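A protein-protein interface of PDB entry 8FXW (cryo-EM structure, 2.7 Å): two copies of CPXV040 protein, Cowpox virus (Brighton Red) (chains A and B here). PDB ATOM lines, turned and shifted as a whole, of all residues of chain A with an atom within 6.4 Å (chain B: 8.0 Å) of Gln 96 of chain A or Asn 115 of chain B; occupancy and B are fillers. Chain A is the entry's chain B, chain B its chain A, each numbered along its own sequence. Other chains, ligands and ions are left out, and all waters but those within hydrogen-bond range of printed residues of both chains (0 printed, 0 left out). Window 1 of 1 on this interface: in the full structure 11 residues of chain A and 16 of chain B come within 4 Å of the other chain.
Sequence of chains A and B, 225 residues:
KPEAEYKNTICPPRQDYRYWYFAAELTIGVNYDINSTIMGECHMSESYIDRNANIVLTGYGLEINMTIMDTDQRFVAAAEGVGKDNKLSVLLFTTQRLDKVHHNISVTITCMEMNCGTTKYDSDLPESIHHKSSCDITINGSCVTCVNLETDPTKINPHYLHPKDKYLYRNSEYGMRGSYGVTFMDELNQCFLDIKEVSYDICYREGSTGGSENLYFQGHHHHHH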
ATOM      1  N   TYR A   6      -1.062   7.776   4.581  1.00  0.00           N
ATOM      2  CA  TYR A   6       0.073   8.036   3.704  1.00  0.00           C
ATOM      3  C   TYR A   6      -0.368   8.140   2.249  1.00  0.00           C
ATOM      4  O   TYR A   6      -1.160   7.326   1.765  1.00  0.00           O
ATOM      5  CB  TYR A   6       1.113   6.928   3.859  1.00  0.00           C
ATOM      6  CG  TYR A   6       2.251   7.035   2.876  1.00  0.00           C
ATOM      7  CD1 TYR A   6       3.267   7.958   3.061  1.00  0.00           C
ATOM      8  CD2 TYR A   6       2.307   6.215   1.764  1.00  0.00           C
ATOM      9  CE1 TYR A   6       4.302   8.063   2.165  1.00  0.00           C
ATOM     10  CE2 TYR A   6       3.340   6.312   0.864  1.00  0.00           C
ATOM     11  CZ  TYR A   6       4.334   7.238   1.068  1.00  0.00           C
ATOM     12  OH  TYR A   6       5.370   7.338   0.171  1.00  0.00           O
ATOM     13  N   ASN A   8       1.519   9.218  -1.725  1.00  0.00           N
ATOM     14  CA  ASN A   8       2.719   9.601  -2.456  1.00  0.00           C
ATOM     15  C   ASN A   8       2.602  11.032  -2.965  1.00  0.00           C
ATOM     16  O   ASN A   8       1.540  11.464  -3.419  1.00  0.00           O
ATOM     17  CB  ASN A   8       2.960   8.652  -3.625  1.00  0.00           C
ATOM     18  CG  ASN A   8       3.480   7.304  -3.182  1.00  0.00           C
ATOM     19  OD1 ASN A   8       2.709   6.380  -2.932  1.00  0.00           O
ATOM     20  ND2 ASN A   8       4.796   7.183  -3.085  1.00  0.00           N
ATOM     21  N   THR A   9       3.705  11.769  -2.881  1.00  0.00           N
ATOM     22  CA  THR A   9       3.750  13.160  -3.295  1.00  0.00           C
ATOM     23  C   THR A   9       4.901  13.366  -4.265  1.00  0.00           C
ATOM     24  O   THR A   9       5.927  12.687  -4.194  1.00  0.00           O
ATOM     25  CB  THR A   9       3.915  14.105  -2.097  1.00  0.00           C
ATOM     26  OG1 THR A   9       5.226  13.954  -1.540  1.00  0.00           O
ATOM     27  CG2 THR A   9       2.878  13.795  -1.032  1.00  0.00           C
ATOM     28  N   TYR A  19      17.384  10.988 -11.799  1.00  0.00           N
ATOM     29  CA  TYR A  19      16.442   9.916 -12.091  1.00  0.00           C
ATOM     30  C   TYR A  19      15.419  10.422 -13.097  1.00  0.00           C
ATOM     31  O   TYR A  19      14.572  11.256 -12.762  1.00  0.00           O
ATOM     32  CB  TYR A  19      15.755   9.438 -10.811  1.00  0.00           C
ATOM     33  CG  TYR A  19      16.720   8.914  -9.775  1.00  0.00           C
ATOM     34  CD1 TYR A  19      17.434   9.780  -8.964  1.00  0.00           C
ATOM     35  CD2 TYR A  19      16.919   7.552  -9.612  1.00  0.00           C
ATOM     36  CE1 TYR A  19      18.319   9.307  -8.022  1.00  0.00           C
ATOM     37  CE2 TYR A  19      17.801   7.069  -8.672  1.00  0.00           C
ATOM     38  CZ  TYR A  19      18.498   7.951  -7.879  1.00  0.00           C
ATOM     39  OH  TYR A  19      19.380   7.474  -6.937  1.00  0.00           O
ATOM     40  N   TRP A  20      15.494   9.912 -14.325  1.00  0.00           N
ATOM     41  CA  TRP A  20      14.701  10.394 -15.444  1.00  0.00           C
ATOM     42  C   TRP A  20      13.722   9.321 -15.891  1.00  0.00           C
ATOM     43  O   TRP A  20      14.056   8.132 -15.914  1.00  0.00           O
ATOM     44  CB  TRP A  20      15.597  10.775 -16.617  1.00  0.00           C
ATOM     45  CG  TRP A  20      16.494  11.939 -16.370  1.00  0.00           C
ATOM     46  CD1 TRP A  20      16.603  12.668 -15.226  1.00  0.00           C
ATOM     47  CD2 TRP A  20      17.411  12.514 -17.302  1.00  0.00           C
ATOM     48  NE1 TRP A  20      17.533  13.662 -15.387  1.00  0.00           N
ATOM     49  CE2 TRP A  20      18.046  13.588 -16.654  1.00  0.00           C
ATOM     50  CE3 TRP A  20      17.757  12.224 -18.623  1.00  0.00           C
ATOM     51  CZ2 TRP A  20      19.004  14.372 -17.283  1.00  0.00           C
ATOM     52  CZ3 TRP A  20      18.707  12.998 -19.243  1.00  0.00           C
ATOM     53  CH2 TRP A  20      19.321  14.062 -18.576  1.00  0.00           C
ATOM     54  N   TYR A  21      12.514   9.747 -16.250  1.00  0.00           N
ATOM     55  CA  TYR A  21      11.493   8.875 -16.808  1.00  0.00           C
ATOM     56  C   TYR A  21      11.161   9.353 -18.212  1.00  0.00           C
ATOM     57  O   TYR A  21      10.846  10.531 -18.410  1.00  0.00           O
ATOM     58  CB  TYR A  21      10.242   8.873 -15.931  1.00  0.00           C
ATOM     59  CG  TYR A  21       9.072   8.148 -16.540  1.00  0.00           C
ATOM     60  CD1 TYR A  21       9.049   6.764 -16.604  1.00  0.00           C
ATOM     61  CD2 TYR A  21       7.988   8.844 -17.048  1.00  0.00           C
ATOM     62  CE1 TYR A  21       7.982   6.096 -17.161  1.00  0.00           C
ATOM     63  CE2 TYR A  21       6.917   8.185 -17.606  1.00  0.00           C
ATOM     64  CZ  TYR A  21       6.919   6.810 -17.659  1.00  0.00           C
ATOM     65  OH  TYR A  21       5.853   6.145 -18.213  1.00  0.00           O
ATOM     66  N   ASP A  72       1.081  14.633 -11.801  1.00  0.00           N
ATOM     67  CA  ASP A  72       2.003  14.550 -10.679  1.00  0.00           C
ATOM     68  C   ASP A  72       3.450  14.432 -11.135  1.00  0.00           C
ATOM     69  O   ASP A  72       4.318  14.066 -10.338  1.00  0.00           O
ATOM     70  CB  ASP A  72       1.640  13.368  -9.778  1.00  0.00           C
ATOM     71  CG  ASP A  72       0.372  13.605  -8.987  1.00  0.00           C
ATOM     72  OD1 ASP A  72       0.082  14.775  -8.662  1.00  0.00           O
ATOM     73  OD2 ASP A  72      -0.334  12.622  -8.685  1.00  0.00           O
ATOM     74  N   GLN A  73       3.722  14.728 -12.401  1.00  0.00           N
ATOM     75  CA  GLN A  73       5.060  14.664 -12.963  1.00  0.00           C
ATOM     76  C   GLN A  73       5.614  16.065 -13.169  1.00  0.00           C
ATOM     77  O   GLN A  73       4.875  17.046 -13.275  1.00  0.00           O
ATOM     78  CB  GLN A  73       5.057  13.915 -14.298  1.00  0.00           C
ATOM     79  CG  GLN A  73       4.527  12.496 -14.223  1.00  0.00           C
ATOM     80  CD  GLN A  73       4.577  11.788 -15.559  1.00  0.00           C
ATOM     81  OE1 GLN A  73       5.068  10.666 -15.659  1.00  0.00           O
ATOM     82  NE2 GLN A  73       4.065  12.439 -16.596  1.00  0.00           N
ATOM     83  N   ARG A  74       6.940  16.142 -13.225  1.00  0.00           N
ATOM     84  CA  ARG A  74       7.649  17.385 -13.490  1.00  0.00           C
ATOM     85  C   ARG A  74       8.715  17.108 -14.536  1.00  0.00           C
ATOM     86  O   ARG A  74       9.450  16.122 -14.425  1.00  0.00           O
ATOM     87  CB  ARG A  74       8.280  17.940 -12.203  1.00  0.00           C
ATOM     88  CG  ARG A  74       9.283  19.065 -12.412  1.00  0.00           C
ATOM     89  CD  ARG A  74      10.034  19.406 -11.134  1.00  0.00           C
ATOM     90  NE  ARG A  74       9.357  20.421 -10.333  1.00  0.00           N
ATOM     91  CZ  ARG A  74       8.591  20.173  -9.278  1.00  0.00           C
ATOM     92  NH1 ARG A  74       8.368  18.940  -8.856  1.00  0.00           N
ATOM     93  NH2 ARG A  74       8.037  21.191  -8.628  1.00  0.00           N
ATOM     94  N   THR A  94      10.734  13.311 -17.568  1.00  0.00           N
ATOM     95  CA  THR A  94      10.054  13.823 -16.391  1.00  0.00           C
ATOM     96  C   THR A  94      10.513  13.051 -15.158  1.00  0.00           C
ATOM     97  O   THR A  94      11.450  12.244 -15.212  1.00  0.00           O
ATOM     98  CB  THR A  94       8.537  13.714 -16.564  1.00  0.00           C
ATOM     99  OG1 THR A  94       8.174  12.345 -16.778  1.00  0.00           O
ATOM    100  CG2 THR A  94       8.057  14.552 -17.732  1.00  0.00           C
ATOM    101  N   THR A  95       9.855  13.311 -14.033  1.00  0.00           N
ATOM    102  CA  THR A  95      10.016  12.490 -12.842  1.00  0.00           C
ATOM    103  C   THR A  95       9.211  11.207 -13.032  1.00  0.00           C
ATOM    104  O   THR A  95       8.641  10.959 -14.097  1.00  0.00           O
ATOM    105  CB  THR A  95       9.592  13.265 -11.596  1.00  0.00           C
ATOM    106  OG1 THR A  95       8.207  13.615 -11.695  1.00  0.00           O
ATOM    107  CG2 THR A  95      10.421  14.527 -11.444  1.00  0.00           C
ATOM    108  N   GLN A  96       9.143  10.375 -12.000  1.00  0.00           N
ATOM    109  CA  GLN A  96       8.467   9.094 -12.139  1.00  0.00           C
ATOM    110  C   GLN A  96       6.961   9.285 -12.283  1.00  0.00           C
ATOM    111  O   GLN A  96       6.417  10.359 -12.018  1.00  0.00           O
ATOM    112  CB  GLN A  96       8.775   8.188 -10.946  1.00  0.00           C
ATOM    113  CG  GLN A  96       8.490   8.801  -9.593  1.00  0.00           C
ATOM    114  CD  GLN A  96       8.698   7.818  -8.462  1.00  0.00           C
ATOM    115  OE1 GLN A  96       9.143   6.691  -8.676  1.00  0.00           O
ATOM    116  NE2 GLN A  96       8.371   8.237  -7.248  1.00  0.00           N
ATOM    117  N   ARG A  97       6.291   8.219 -12.713  1.00  0.00           N
ATOM    118  CA  ARG A  97       4.865   8.244 -13.024  1.00  0.00           C
ATOM    119  C   ARG A  97       4.112   7.631 -11.850  1.00  0.00           C
ATOM    120  O   ARG A  97       4.063   6.408 -11.700  1.00  0.00           O
ATOM    121  CB  ARG A  97       4.602   7.483 -14.319  1.00  0.00           C
ATOM    122  CG  ARG A  97       3.169   7.526 -14.828  1.00  0.00           C
ATOM    123  CD  ARG A  97       2.971   8.604 -15.881  1.00  0.00           C
ATOM    124  NE  ARG A  97       1.938   8.241 -16.843  1.00  0.00           N
ATOM    125  CZ  ARG A  97       0.636   8.385 -16.639  1.00  0.00           C
ATOM    126  NH1 ARG A  97       0.162   8.876 -15.506  1.00  0.00           N
ATOM    127  NH2 ARG A  97      -0.213   8.024 -17.597  1.00  0.00           N
ATOM    128  N   LEU A  98       3.522   8.482 -11.010  1.00  0.00           N
ATOM    129  CA  LEU A  98       2.819   7.987  -9.832  1.00  0.00           C
ATOM    130  C   LEU A  98       1.494   7.325 -10.191  1.00  0.00           C
ATOM    131  O   LEU A  98       1.192   6.235  -9.692  1.00  0.00           O
ATOM    132  CB  LEU A  98       2.584   9.128  -8.844  1.00  0.00           C
ATOM    133  CG  LEU A  98       3.836   9.810  -8.293  1.00  0.00           C
ATOM    134  CD1 LEU A  98       3.448  10.905  -7.320  1.00  0.00           C
ATOM    135  CD2 LEU A  98       4.758   8.806  -7.624  1.00  0.00           C
ATOM    136  N   ASP A  99       0.697   7.955 -11.046  1.00  0.00           N
ATOM    137  CA  ASP A  99      -0.633   7.465 -11.377  1.00  0.00           C
ATOM    138  C   ASP A  99      -0.670   6.932 -12.802  1.00  0.00           C
ATOM    139  O   ASP A  99       0.007   7.445 -13.696  1.00  0.00           O
ATOM    140  CB  ASP A  99      -1.681   8.570 -11.212  1.00  0.00           C
ATOM    141  CG  ASP A  99      -1.372   9.797 -12.043  1.00  0.00           C
ATOM    142  OD1 ASP A  99      -0.283   9.850 -12.650  1.00  0.00           O
ATOM    143  OD2 ASP A  99      -2.220  10.712 -12.088  1.00  0.00           O
ATOM    144  N   VAL B  30      17.441   1.221   0.705  1.00  0.00           N
ATOM    145  CA  VAL B  30      16.462   1.899  -0.133  1.00  0.00           C
ATOM    146  C   VAL B  30      15.956   0.929  -1.193  1.00  0.00           C
ATOM    147  O   VAL B  30      16.596  -0.075  -1.511  1.00  0.00           O
ATOM    148  CB  VAL B  30      17.043   3.166  -0.792  1.00  0.00           C
ATOM    149  CG1 VAL B  30      17.477   4.158   0.267  1.00  0.00           C
ATOM    150  CG2 VAL B  30      18.206   2.815  -1.703  1.00  0.00           C
ATOM    151  N   ASN B  31      14.785   1.246  -1.742  1.00  0.00           N
ATOM    152  CA  ASN B  31      14.174   0.452  -2.797  1.00  0.00           C
ATOM    153  C   ASN B  31      14.413   1.030  -4.187  1.00  0.00           C
ATOM    154  O   ASN B  31      13.817   0.550  -5.155  1.00  0.00           O
ATOM    155  CB  ASN B  31      12.672   0.301  -2.548  1.00  0.00           C
ATOM    156  CG  ASN B  31      11.949   1.626  -2.519  1.00  0.00           C
ATOM    157  OD1 ASN B  31      12.510   2.665  -2.859  1.00  0.00           O
ATOM    158  ND2 ASN B  31      10.687   1.597  -2.112  1.00  0.00           N
ATOM    159  N   TYR B  32      15.260   2.049  -4.309  1.00  0.00           N
ATOM    160  CA  TYR B  32      15.652   2.589  -5.599  1.00  0.00           C
ATOM    161  C   TYR B  32      17.159   2.456  -5.766  1.00  0.00           C
ATOM    162  O   TYR B  32      17.888   2.162  -4.817  1.00  0.00           O
ATOM    163  CB  TYR B  32      15.219   4.051  -5.760  1.00  0.00           C
ATOM    164  CG  TYR B  32      15.762   4.998  -4.721  1.00  0.00           C
ATOM    165  CD1 TYR B  32      15.108   5.177  -3.513  1.00  0.00           C
ATOM    166  CD2 TYR B  32      16.915   5.728  -4.954  1.00  0.00           C
ATOM    167  CE1 TYR B  32      15.594   6.047  -2.565  1.00  0.00           C
ATOM    168  CE2 TYR B  32      17.408   6.600  -4.013  1.00  0.00           C
ATOM    169  CZ  TYR B  32      16.744   6.757  -2.820  1.00  0.00           C
ATOM    170  OH  TYR B  32      17.233   7.626  -1.874  1.00  0.00           O
ATOM    171  N   ASP B  33      17.619   2.678  -6.993  1.00  0.00           N
ATOM    172  CA  ASP B  33      18.974   2.304  -7.377  1.00  0.00           C
ATOM    173  C   ASP B  33      19.981   3.357  -6.935  1.00  0.00           C
ATOM    174  O   ASP B  33      19.845   4.539  -7.266  1.00  0.00           O
ATOM    175  CB  ASP B  33      19.054   2.100  -8.886  1.00  0.00           C
ATOM    176  CG  ASP B  33      18.542   0.749  -9.311  1.00  0.00           C
ATOM    177  OD1 ASP B  33      17.356   0.454  -9.058  1.00  0.00           O
ATOM    178  OD2 ASP B  33      19.323  -0.025  -9.899  1.00  0.00           O
ATOM    179  N   GLY B  61      19.888  10.999  -2.591  1.00  0.00           N
ATOM    180  CA  GLY B  61      18.444  11.060  -2.592  1.00  0.00           C
ATOM    181  C   GLY B  61      17.797  10.973  -1.232  1.00  0.00           C
ATOM    182  O   GLY B  61      16.576  10.799  -1.158  1.00  0.00           O
ATOM    183  N   THR B 110      14.144  11.147   5.406  1.00  0.00           N
ATOM    184  CA  THR B 110      13.209  11.747   4.467  1.00  0.00           C
ATOM    185  C   THR B 110      13.690  11.499   3.047  1.00  0.00           C
ATOM    186  O   THR B 110      14.870  11.692   2.739  1.00  0.00           O
ATOM    187  CB  THR B 110      13.069  13.255   4.712  1.00  0.00           C
ATOM    188  OG1 THR B 110      12.327  13.481   5.917  1.00  0.00           O
ATOM    189  CG2 THR B 110      12.367  13.930   3.550  1.00  0.00           C
ATOM    190  N   CYS B 111      12.775  11.070   2.183  1.00  0.00           N
ATOM    191  CA  CYS B 111      13.121  10.875   0.783  1.00  0.00           C
ATOM    192  C   CYS B 111      13.027  12.190   0.019  1.00  0.00           C
ATOM    193  O   CYS B 111      12.179  13.038   0.302  1.00  0.00           O
ATOM    194  CB  CYS B 111      12.207   9.846   0.134  1.00  0.00           C
ATOM    195  SG  CYS B 111      12.095   8.276   0.995  1.00  0.00           S
ATOM    196  N   MET B 112      13.912  12.348  -0.965  1.00  0.00           N
ATOM    197  CA  MET B 112      14.016  13.595  -1.711  1.00  0.00           C
ATOM    198  C   MET B 112      14.131  13.428  -3.219  1.00  0.00           C
ATOM    199  O   MET B 112      14.027  14.434  -3.929  1.00  0.00           O
ATOM    200  CB  MET B 112      15.225  14.406  -1.222  1.00  0.00           C
ATOM    201  CG  MET B 112      15.182  14.754   0.258  1.00  0.00           C
ATOM    202  SD  MET B 112      13.789  15.804   0.710  1.00  0.00           S
ATOM    203  CE  MET B 112      14.222  17.329  -0.121  1.00  0.00           C
ATOM    204  N   GLU B 113      14.338  12.220  -3.735  1.00  0.00           N
ATOM    205  CA  GLU B 113      14.522  12.026  -5.169  1.00  0.00           C
ATOM    206  C   GLU B 113      13.699  10.888  -5.748  1.00  0.00           C
ATOM    207  O   GLU B 113      13.439  10.882  -6.953  1.00  0.00           O
ATOM    208  CB  GLU B 113      16.005  11.783  -5.476  1.00  0.00           C
ATOM    209  CG  GLU B 113      16.877  13.003  -5.255  1.00  0.00           C
ATOM    210  CD  GLU B 113      18.325  12.762  -5.624  1.00  0.00           C
ATOM    211  OE1 GLU B 113      18.646  11.648  -6.084  1.00  0.00           O
ATOM    212  OE2 GLU B 113      19.146  13.686  -5.451  1.00  0.00           O
ATOM    213  N   MET B 114      13.275   9.926  -4.934  1.00  0.00           N
ATOM    214  CA  MET B 114      12.473   8.809  -5.409  1.00  0.00           C
ATOM    215  C   MET B 114      11.527   8.346  -4.313  1.00  0.00           C
ATOM    216  O   MET B 114      11.913   8.225  -3.148  1.00  0.00           O
ATOM    217  CB  MET B 114      13.352   7.636  -5.861  1.00  0.00           C
ATOM    218  CG  MET B 114      14.091   7.871  -7.169  1.00  0.00           C
ATOM    219  SD  MET B 114      13.006   7.926  -8.609  1.00  0.00           S
ATOM    220  CE  MET B 114      12.413   6.240  -8.667  1.00  0.00           C
ATOM    221  N   ASN B 115      10.282   8.091  -4.702  1.00  0.00           N
ATOM    222  CA  ASN B 115       9.264   7.546  -3.807  1.00  0.00           C
ATOM    223  C   ASN B 115       9.018   8.472  -2.619  1.00  0.00           C
ATOM    224  O   ASN B 115       8.965   8.048  -1.464  1.00  0.00           O
ATOM    225  CB  ASN B 115       9.651   6.145  -3.341  1.00  0.00           C
ATOM    226  CG  ASN B 115       9.751   5.160  -4.483  1.00  0.00           C
ATOM    227  OD1 ASN B 115       8.742   4.665  -4.978  1.00  0.00           O
ATOM    228  ND2 ASN B 115      10.974   4.867  -4.906  1.00  0.00           N
ATOM    229  N   CYS B 116       8.847   9.756  -2.915  1.00  0.00           N
ATOM    230  CA  CYS B 116       8.570  10.732  -1.873  1.00  0.00           C
ATOM    231  C   CYS B 116       7.126  10.605  -1.392  1.00  0.00           C
ATOM    232  O   CYS B 116       6.273   9.988  -2.035  1.00  0.00           O
ATOM    233  CB  CYS B 116       8.836  12.146  -2.380  1.00  0.00           C
ATOM    234  SG  CYS B 116      10.530  12.420  -2.927  1.00  0.00           S
ATOM    235  N   GLY B 117       6.860  11.206  -0.240  1.00  0.00           N
ATOM    236  CA  GLY B 117       5.541  11.143   0.350  1.00  0.00           C
ATOM    237  C   GLY B 117       5.534  11.831   1.699  1.00  0.00           C
ATOM    238  O   GLY B 117       6.516  12.458   2.102  1.00  0.00           O
ATOM    239  N   THR B 118       4.403  11.704   2.387  1.00  0.00           N
ATOM    240  CA  THR B 118       4.253  12.242   3.729  1.00  0.00           C
ATOM    241  C   THR B 118       4.736  11.201   4.737  1.00  0.00           C
ATOM    242  O   THR B 118       5.263  10.148   4.371  1.00  0.00           O
ATOM    243  CB  THR B 118       2.803  12.654   3.983  1.00  0.00           C
ATOM    244  OG1 THR B 118       1.933  11.538   3.759  1.00  0.00           O
ATOM    245  CG2 THR B 118       2.406  13.792   3.066  1.00  0.00           C
ATOM    246  N   LYS B 120       5.359   8.240   6.576  1.00  0.00           N
ATOM    247  CA  LYS B 120       4.951   6.851   6.437  1.00  0.00           C
ATOM    248  C   LYS B 120       5.178   6.040   7.699  1.00  0.00           C
ATOM    249  O   LYS B 120       4.430   5.091   7.950  1.00  0.00           O
ATOM    250  CB  LYS B 120       5.697   6.183   5.278  1.00  0.00           C
ATOM    251  CG  LYS B 120       5.263   4.751   5.035  1.00  0.00           C
ATOM    252  CD  LYS B 120       5.714   4.236   3.683  1.00  0.00           C
ATOM    253  CE  LYS B 120       5.071   2.895   3.373  1.00  0.00           C
ATOM    254  NZ  LYS B 120       5.449   2.382   2.027  1.00  0.00           N
ATOM    255  N   ILE B 139      10.077   8.091   9.350  1.00  0.00           N
ATOM    256  CA  ILE B 139      10.366   7.915   7.929  1.00  0.00           C
ATOM    257  C   ILE B 139       9.290   8.639   7.132  1.00  0.00           C
ATOM    258  O   ILE B 139       8.097   8.326   7.257  1.00  0.00           O
ATOM    259  CB  ILE B 139      10.429   6.431   7.536  1.00  0.00           C
ATOM    260  CG1 ILE B 139      11.628   5.744   8.190  1.00  0.00           C
ATOM    261  CG2 ILE B 139      10.497   6.287   6.021  1.00  0.00           C
ATOM    262  CD1 ILE B 139      11.329   5.160   9.548  1.00  0.00           C
ATOM    263  N   ASN B 140       9.727   9.597   6.306  1.00  0.00           N
ATOM    264  CA  ASN B 140       8.876  10.380   5.409  1.00  0.00           C
ATOM    265  C   ASN B 140       9.151   9.925   3.979  1.00  0.00           C
ATOM    266  O   ASN B 140      10.112  10.378   3.343  1.00  0.00           O
ATOM    267  CB  ASN B 140       9.143  11.875   5.562  1.00  0.00           C
ATOM    268  CG  ASN B 140       8.289  12.518   6.629  1.00  0.00           C
ATOM    269  OD1 ASN B 140       7.928  11.883   7.619  1.00  0.00           O
ATOM    270  ND2 ASN B 140       7.959  13.788   6.434  1.00  0.00           N
ATOM    271  N   GLY B 141       8.297   9.041   3.478  1.00  0.00           N
ATOM    272  CA  GLY B 141       8.396   8.502   2.142  1.00  0.00           C
ATOM    273  C   GLY B 141       8.123   7.016   2.125  1.00  0.00           C
ATOM    274  O   GLY B 141       7.796   6.402   3.138  1.00  0.00           O
ATOM    275  N   SER B 142       8.266   6.434   0.936  1.00  0.00           N
ATOM    276  CA  SER B 142       8.116   4.997   0.740  1.00  0.00           C
ATOM    277  C   SER B 142       9.354   4.379   0.106  1.00  0.00           C
ATOM    278  O   SER B 142       9.238   3.531  -0.784  1.00  0.00           O
ATOM    279  CB  SER B 142       6.883   4.706  -0.114  1.00  0.00           C
ATOM    280  OG  SER B 142       6.959   5.370  -1.362  1.00  0.00           O
ATOM    281  N   CYS B 143      10.539   4.790   0.552  1.00  0.00           N
ATOM    282  CA  CYS B 143      11.802   4.380  -0.044  1.00  0.00           C
ATOM    283  C   CYS B 143      12.624   3.512   0.894  1.00  0.00           C
ATOM    284  O   CYS B 143      13.375   2.645   0.440  1.00  0.00           O
ATOM    285  CB  CYS B 143      12.587   5.628  -0.440  1.00  0.00           C
ATOM    286  SG  CYS B 143      11.482   7.039  -0.488  1.00  0.00           S
ATOM    287  N   VAL B 144      12.488   3.731   2.200  1.00  0.00           N
ATOM    288  CA  VAL B 144      13.265   2.981   3.175  1.00  0.00           C
ATOM    289  C   VAL B 144      12.656   1.600   3.356  1.00  0.00           C
ATOM    290  O   VAL B 144      11.442   1.459   3.557  1.00  0.00           O
ATOM    291  CB  VAL B 144      13.327   3.746   4.505  1.00  0.00           C
ATOM    292  CG1 VAL B 144      13.928   2.879   5.589  1.00  0.00           C
ATOM    293  CG2 VAL B 144      14.133   5.019   4.339  1.00  0.00           C
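Of the 15 printed residues of chain A, 5 touch a printed residue of chain B. Printed residues of chain A that touch a printed residue of chain B: Tyr 6, Asn 8, Thr 9, Tyr 19 and Gln 96. Printed residues of chain B that touch a printed residue of chain A: Tyr 32, Asp 33, Glu 113, Met 114, Asn 115, Cys 116, Gly 117, Thr 118, Lys 120, Gly 141 and Ser 142. Among the printed residues, no Asp or Glu carboxylate lies within 4 Å of a Lys or Arg side-chain nitrogen of the other chain.
OD1 of Asn 31 of chain B is in hydrogen-bond range of ND2 of Asn 115 of chain B, at 3.4 Å. ND2 of Asn 31 of chain B lies within hydrogen-bond range of O of Ser 142 of chain B, 2.8 Å away. O of Cys 111 of chain B is in hydrogen-bond range of SG of Cys 116 of chain B (3.7 Å). The backbone carbonyl oxygen (O) of Asn 115 of chain B sits at hydrogen-bond distance from the backbone NH (N) of Ser 142 of chain B. OH of Tyr 6 of chain A is in hydrogen-bond range of ND2 of Asn 8 of chain A (3.3 Å). The side-chain sulfur of Cys 111 of chain B is disulfide-bonded to the side-chain sulfur of Cys 143 of chain B, at 2.0 Å.
Printed residues of chain B within 4 Å of Thr 9 of chain A: Cys 116 and Gly 117. Gln 96 of chain A touches two residues of chain B. Printed residues of chain A within 4 Å of Glu 113 of chain B: Tyr 19. Printed residues of chain A within 4 Å of Asn 115 of chain B: Gln 96 (3.2 Å). Printed residues of chain A within 4 Å of Gly 141 of chain B: Tyr 6. The nearest residue of chain B that does not touch Gln 96 of chain A is Cys 116 of chain B (4.6 Å). The nearest printed residue of chain A that does not touch Gly 117 of chain B is Asn 8 of chain A (4.3 Å).
No position is printed for both chains.
Among the printed residues, merely in contact across the chains: Tyr 19 of chain A with Glu 113 of chain B (3.1 Å), Tyr 6 of chain A with Thr 118 of chain B (3.2 Å), Gln 96 of chain A with Met 114 of chain B (3.3 Å), Tyr 6 of chain A with Gly 141 of chain B (3.4 Å), Tyr 6 of chain A with Cys 116 of chain B (3.6 Å), Tyr 19 of chain A with Tyr 32 of chain B (3.6 Å), Tyr 6 of chain A with Lys 120 of chain B (3.7 Å), Tyr 19 of chain A with Met 114 of chain B (3.8 Å) and Tyr 6 of chain A with Gly 117 of chain B (3.8 Å).
O of Asp 33 of chain B is in hydrogen-bond range of OH of Tyr 19 of chain A (3.0 Å). The side-chain amide nitrogen (NE2) of Gln 96 of chain A lies close to the backbone NH (N) of Asn 115 of chain B, 3.2 Å away. The side-chain amide nitrogen of Asn 8 of chain A lies within hydrogen-bond range of the backbone carbonyl oxygen of Cys 116 of chain B, 3.3 Å away. O of Cys 116 of chain B sits at hydrogen-bond distance from N of Thr 9 of chain A, at 3.2 Å. The backbone NH (N) of Gly 117 of chain B sits close to the side-chain hydroxyl (OG1) of Thr 9 of chain A, 3.5 Å away. The side-chain hydroxyl (OG) of Ser 142 of chain B lies within hydrogen-bond range of the side-chain hydroxyl (OH) of Tyr 6 of chain A, 3.0 Å away. OG of Ser 142 of chain B sits at hydrogen-bond distance from ND2 of Asn 8 of chain A, at 3.3 Å.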
